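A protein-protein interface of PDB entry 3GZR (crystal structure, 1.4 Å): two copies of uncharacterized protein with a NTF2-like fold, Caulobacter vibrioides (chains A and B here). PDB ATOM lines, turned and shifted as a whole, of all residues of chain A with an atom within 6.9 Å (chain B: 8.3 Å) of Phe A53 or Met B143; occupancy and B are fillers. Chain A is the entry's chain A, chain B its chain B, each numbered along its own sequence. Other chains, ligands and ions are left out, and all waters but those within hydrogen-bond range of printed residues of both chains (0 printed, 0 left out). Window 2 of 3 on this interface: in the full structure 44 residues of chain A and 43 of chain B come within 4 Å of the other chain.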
ATOM      1  N   ARG A  48     -30.289 -10.764 -11.331  1.00  0.00           N
ATOM      2  CA  ARG A  48     -29.265  -9.792 -11.759  1.00  0.00           C
ATOM      3  C   ARG A  48     -27.906 -10.406 -12.088  1.00  0.00           C
ATOM      4  O   ARG A  48     -27.292  -9.987 -13.080  1.00  0.00           O
ATOM      5  CB  ARG A  48     -29.088  -8.698 -10.722  1.00  0.00           C
ATOM      6  CG  ARG A  48     -28.144  -7.593 -11.157  1.00  0.00           C
ATOM      7  CD  ARG A  48     -28.113  -6.483 -10.156  1.00  0.00           C
ATOM      8  NE  ARG A  48     -27.628  -6.881  -8.845  1.00  0.00           N
ATOM      9  CZ  ARG A  48     -27.490  -6.054  -7.818  1.00  0.00           C
ATOM     10  NH1 ARG A  48     -27.771  -4.768  -7.932  1.00  0.00           N
ATOM     11  NH2 ARG A  48     -27.020  -6.506  -6.654  1.00  0.00           N
ATOM     12  N   ASP A  49     -27.467 -11.387 -11.309  1.00  0.00           N
ATOM     13  CA  ASP A  49     -26.143 -11.929 -11.557  1.00  0.00           C
ATOM     14  C   ASP A  49     -26.077 -12.529 -12.962  1.00  0.00           C
ATOM     15  O   ASP A  49     -25.060 -12.362 -13.649  1.00  0.00           O
ATOM     16  CB  ASP A  49     -25.743 -12.967 -10.514  1.00  0.00           C
ATOM     17  CG  ASP A  49     -25.307 -12.348  -9.178  1.00  0.00           C
ATOM     18  OD1 ASP A  49     -25.089 -11.116  -9.052  1.00  0.00           O
ATOM     19  OD2 ASP A  49     -25.078 -13.178  -8.250  1.00  0.00           O
ATOM     20  N   GLN A  50     -27.125 -13.230 -13.376  1.00  0.00           N
ATOM     21  CA  GLN A  50     -27.194 -13.803 -14.747  1.00  0.00           C
ATOM     22  C   GLN A  50     -27.197 -12.709 -15.822  1.00  0.00           C
ATOM     23  O   GLN A  50     -26.487 -12.796 -16.829  1.00  0.00           O
ATOM     24  CB  GLN A  50     -28.413 -14.710 -14.917  1.00  0.00           C
ATOM     25  CG  GLN A  50     -28.268 -16.069 -14.209  1.00  0.00           C
ATOM     26  CD  GLN A  50     -29.388 -17.032 -14.510  1.00  0.00           C
ATOM     27  OE1 GLN A  50     -30.107 -16.895 -15.503  1.00  0.00           O
ATOM     28  NE2 GLN A  50     -29.494 -18.095 -13.685  1.00  0.00           N
ATOM     29  N   ILE A  51     -27.990 -11.670 -15.583  1.00  0.00           N
ATOM     30  CA  ILE A  51     -28.073 -10.528 -16.528  1.00  0.00           C
ATOM     31  C   ILE A  51     -26.692  -9.941 -16.757  1.00  0.00           C
ATOM     32  O   ILE A  51     -26.244  -9.784 -17.901  1.00  0.00           O
ATOM     33  CB  ILE A  51     -29.066  -9.438 -16.051  1.00  0.00           C
ATOM     34  CG1 ILE A  51     -30.507  -9.997 -15.936  1.00  0.00           C
ATOM     35  CG2 ILE A  51     -29.041  -8.266 -17.023  1.00  0.00           C
ATOM     36  CD1 ILE A  51     -31.480  -9.011 -15.312  1.00  0.00           C
ATOM     37  N   VAL A  52     -26.003  -9.665 -15.662  1.00  0.00           N
ATOM     38  CA  VAL A  52     -24.687  -9.049 -15.704  1.00  0.00           C
ATOM     39  C   VAL A  52     -23.651  -9.991 -16.303  1.00  0.00           C
ATOM     40  O   VAL A  52     -22.861  -9.552 -17.143  1.00  0.00           O
ATOM     41  CB  VAL A  52     -24.292  -8.540 -14.302  1.00  0.00           C
ATOM     42  CG1 VAL A  52     -22.825  -8.065 -14.263  1.00  0.00           C
ATOM     43  CG2 VAL A  52     -25.237  -7.421 -13.854  1.00  0.00           C
ATOM     44  N   PHE A  53     -23.661 -11.271 -15.925  1.00  0.00           N
ATOM     45  CA  PHE A  53     -22.702 -12.259 -16.443  1.00  0.00           C
ATOM     46  C   PHE A  53     -22.820 -12.358 -17.962  1.00  0.00           C
ATOM     47  O   PHE A  53     -21.843 -12.352 -18.687  1.00  0.00           O
ATOM     48  CB  PHE A  53     -22.944 -13.631 -15.812  1.00  0.00           C
ATOM     49  CG  PHE A  53     -21.877 -14.619 -16.139  1.00  0.00           C
ATOM     50  CD1 PHE A  53     -21.972 -15.425 -17.277  1.00  0.00           C
ATOM     51  CD2 PHE A  53     -20.752 -14.721 -15.325  1.00  0.00           C
ATOM     52  CE1 PHE A  53     -20.965 -16.335 -17.592  1.00  0.00           C
ATOM     53  CE2 PHE A  53     -19.736 -15.621 -15.633  1.00  0.00           C
ATOM     54  CZ  PHE A  53     -19.844 -16.423 -16.780  1.00  0.00           C
ATOM     55  N   ALA A  54     -24.051 -12.430 -18.457  1.00  0.00           N
ATOM     56  CA  ALA A  54     -24.266 -12.576 -19.906  1.00  0.00           C
ATOM     57  C   ALA A  54     -23.929 -11.303 -20.679  1.00  0.00           C
ATOM     58  O   ALA A  54     -23.291 -11.363 -21.730  1.00  0.00           O
ATOM     59  CB  ALA A  54     -25.692 -13.020 -20.193  1.00  0.00           C
ATOM     60  N   HIS A  55     -24.357 -10.155 -20.163  1.00  0.00           N
ATOM     61  CA  HIS A  55     -24.000  -8.872 -20.801  1.00  0.00           C
ATOM     62  C   HIS A  55     -22.491  -8.716 -20.887  1.00  0.00           C
ATOM     63  O   HIS A  55     -21.941  -8.296 -21.929  1.00  0.00           O
ATOM     64  CB  HIS A  55     -24.579  -7.672 -20.043  1.00  0.00           C
ATOM     65  CG  HIS A  55     -25.992  -7.338 -20.392  1.00  0.00           C
ATOM     66  ND1 HIS A  55     -27.066  -8.118 -20.023  1.00  0.00           N
ATOM     67  CD2 HIS A  55     -26.488  -6.323 -21.131  1.00  0.00           C
ATOM     68  CE1 HIS A  55     -28.176  -7.557 -20.487  1.00  0.00           C
ATOM     69  NE2 HIS A  55     -27.854  -6.453 -21.141  1.00  0.00           N
ATOM     70  N   THR A  56     -21.809  -9.049 -19.792  1.00  0.00           N
ATOM     71  CA  THR A  56     -20.347  -8.963 -19.734  1.00  0.00           C
ATOM     72  C   THR A  56     -19.704  -9.895 -20.758  1.00  0.00           C
ATOM     73  O   THR A  56     -18.819  -9.462 -21.507  1.00  0.00           O
ATOM     74  CB  THR A  56     -19.827  -9.282 -18.313  1.00  0.00           C
ATOM     75  OG1 THR A  56     -20.429  -8.363 -17.384  1.00  0.00           O
ATOM     76  CG2 THR A  56     -18.330  -9.147 -18.223  1.00  0.00           C
ATOM     77  N   ALA A  57     -20.179 -11.141 -20.822  1.00  0.00           N
ATOM     78  CA  ALA A  57     -19.628 -12.143 -21.742  1.00  0.00           C
ATOM     79  C   ALA A  57     -19.736 -11.699 -23.183  1.00  0.00           C
ATOM     80  O   ALA A  57     -18.734 -11.784 -23.926  1.00  0.00           O
ATOM     81  CB  ALA A  57     -20.309 -13.477 -21.555  1.00  0.00           C
ATOM     82  N   PHE A  58     -20.895 -11.181 -23.576  1.00  0.00           N
ATOM     83  CA  PHE A  58     -21.083 -10.805 -24.984  1.00  0.00           C
ATOM     84  C   PHE A  58     -20.376  -9.495 -25.325  1.00  0.00           C
ATOM     85  O   PHE A  58     -19.901  -9.340 -26.441  1.00  0.00           O
ATOM     86  CB  PHE A  58     -22.540 -10.769 -25.409  1.00  0.00           C
ATOM     87  CG  PHE A  58     -23.201 -12.120 -25.520  1.00  0.00           C
ATOM     88  CD1 PHE A  58     -22.664 -13.114 -26.342  1.00  0.00           C
ATOM     89  CD2 PHE A  58     -24.402 -12.362 -24.905  1.00  0.00           C
ATOM     90  CE1 PHE A  58     -23.291 -14.337 -26.469  1.00  0.00           C
ATOM     91  CE2 PHE A  58     -25.054 -13.592 -25.079  1.00  0.00           C
ATOM     92  CZ  PHE A  58     -24.487 -14.559 -25.846  1.00  0.00           C
ATOM     93  N   ASP B 138     -25.454 -19.464 -24.878  1.00  0.00           N
ATOM     94  CA  ASP B 138     -25.938 -18.696 -23.737  1.00  0.00           C
ATOM     95  C   ASP B 138     -24.861 -18.723 -22.652  1.00  0.00           C
ATOM     96  O   ASP B 138     -24.524 -19.788 -22.157  1.00  0.00           O
ATOM     97  CB  ASP B 138     -27.261 -19.263 -23.230  1.00  0.00           C
ATOM     98  CG  ASP B 138     -27.903 -18.414 -22.166  1.00  0.00           C
ATOM     99  OD1 ASP B 138     -27.206 -17.645 -21.501  1.00  0.00           O
ATOM    100  OD2 ASP B 138     -29.127 -18.555 -21.976  1.00  0.00           O
ATOM    101  N   PRO B 139     -24.301 -17.552 -22.293  1.00  0.00           N
ATOM    102  CA  PRO B 139     -23.205 -17.537 -21.301  1.00  0.00           C
ATOM    103  C   PRO B 139     -23.554 -18.073 -19.921  1.00  0.00           C
ATOM    104  O   PRO B 139     -22.670 -18.565 -19.242  1.00  0.00           O
ATOM    105  CB  PRO B 139     -22.852 -16.039 -21.196  1.00  0.00           C
ATOM    106  CG  PRO B 139     -23.279 -15.484 -22.465  1.00  0.00           C
ATOM    107  CD  PRO B 139     -24.573 -16.172 -22.752  1.00  0.00           C
ATOM    108  N   VAL B 140     -24.829 -18.033 -19.528  1.00  0.00           N
ATOM    109  CA  VAL B 140     -25.243 -18.492 -18.194  1.00  0.00           C
ATOM    110  C   VAL B 140     -24.977 -19.988 -18.007  1.00  0.00           C
ATOM    111  O   VAL B 140     -24.827 -20.443 -16.887  1.00  0.00           O
ATOM    112  CB  VAL B 140     -26.697 -18.041 -17.891  1.00  0.00           C
ATOM    113  CG1 VAL B 140     -27.295 -18.717 -16.649  1.00  0.00           C
ATOM    114  CG2 VAL B 140     -26.679 -16.546 -17.735  1.00  0.00           C
ATOM    115  N   LEU B 141     -24.899 -20.734 -19.116  1.00  0.00           N
ATOM    116  CA  LEU B 141     -24.511 -22.171 -19.062  1.00  0.00           C
ATOM    117  C   LEU B 141     -23.072 -22.359 -18.508  1.00  0.00           C
ATOM    118  O   LEU B 141     -22.745 -23.445 -17.993  1.00  0.00           O
ATOM    119  CB  LEU B 141     -24.605 -22.796 -20.456  1.00  0.00           C
ATOM    120  CG  LEU B 141     -25.967 -22.792 -21.156  1.00  0.00           C
ATOM    121  CD1 LEU B 141     -25.821 -23.233 -22.626  1.00  0.00           C
ATOM    122  CD2 LEU B 141     -26.992 -23.642 -20.402  1.00  0.00           C
ATOM    123  N   ARG B 142     -22.215 -21.330 -18.621  1.00  0.00           N
ATOM    124  CA  ARG B 142     -20.807 -21.346 -18.147  1.00  0.00           C
ATOM    125  C   ARG B 142     -20.563 -20.778 -16.726  1.00  0.00           C
ATOM    126  O   ARG B 142     -19.414 -20.750 -16.281  1.00  0.00           O
ATOM    127  CB  ARG B 142     -19.914 -20.573 -19.155  1.00  0.00           C
ATOM    128  CG  ARG B 142     -19.983 -21.069 -20.606  1.00  0.00           C
ATOM    129  N   MET B 143     -21.600 -20.331 -16.007  1.00  0.00           N
ATOM    130  CA  MET B 143     -21.394 -19.760 -14.648  1.00  0.00           C
ATOM    131  C   MET B 143     -20.967 -20.774 -13.579  1.00  0.00           C
ATOM    132  O   MET B 143     -21.673 -21.741 -13.326  1.00  0.00           O
ATOM    133  CB  MET B 143     -22.637 -19.013 -14.171  1.00  0.00           C
ATOM    134  CG  MET B 143     -22.821 -17.753 -14.897  1.00  0.00           C
ATOM    135  SD  MET B 143     -24.426 -16.834 -14.361  1.00  0.00           S
ATOM    136  CE  MET B 143     -24.064 -15.960 -12.759  1.00  0.00           C
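Of the 11 printed residues of chain A, 6 touch a printed residue of chain B.
Hydrophobic or aromatic side chains of chain A within 4 Å of the printed part of chain B: Phe A53, Ala A57 and Phe A58.
Printed residues of chain B that touch a printed residue of chain A: Pro B139, Val B140 and Met B143.
Among the printed residues, 8 pairs touch across the chains.
Among the printed residues, no Asp or Glu carboxylate lies within 4 Å of a Lys or Arg side-chain nitrogen of the other chain.
Among the printed residues, pairs that only touch across the chains: Phe A53 with Pro B139 (3.3 Å), Gln A50 with Val B140 (3.4 Å), Phe A53 with Met B143 (3.4 Å), Phe A58 with Pro B139 (3.5 Å), Ala A57 with Pro B139 (3.6 Å), Asp A49 with Met B143 (3.8 Å), Gln A50 with Met B143 (3.9 Å) and Ala A54 with Pro B139 (3.96 Å).
Phe A53 touches just these residues of chain B: Pro B139 and Met B143.
Of chain A, only Asp A49 (3.8 Å), Gln A50 (3.9 Å) and Phe A53 (3.4 Å) come within 4 Å of Met B143.
Of the printed residues of chain B, Ala A54 touches Pro B139.
Of the printed residues of chain A, Pro B139 touches Phe A53, Ala A54, Ala A57 and Phe A58.
Of the printed residues of chain B, Phe A58 touches Pro B139 (3.5 Å).
The nearest residue of chain B that does not touch Phe A53 is Arg B142 (4.4 Å).
The nearest printed residue of chain B that does not touch Gln A50 is Pro B139 (6.5 Å).
OD1 of Asp B138 sits at hydrogen-bond distance from N of Val B140 (3.1 Å).
No position is printed for both chains.
Of the 8 pairs that touch across the chains among the printed residues, none has its exchanged pair printed and touching as well.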
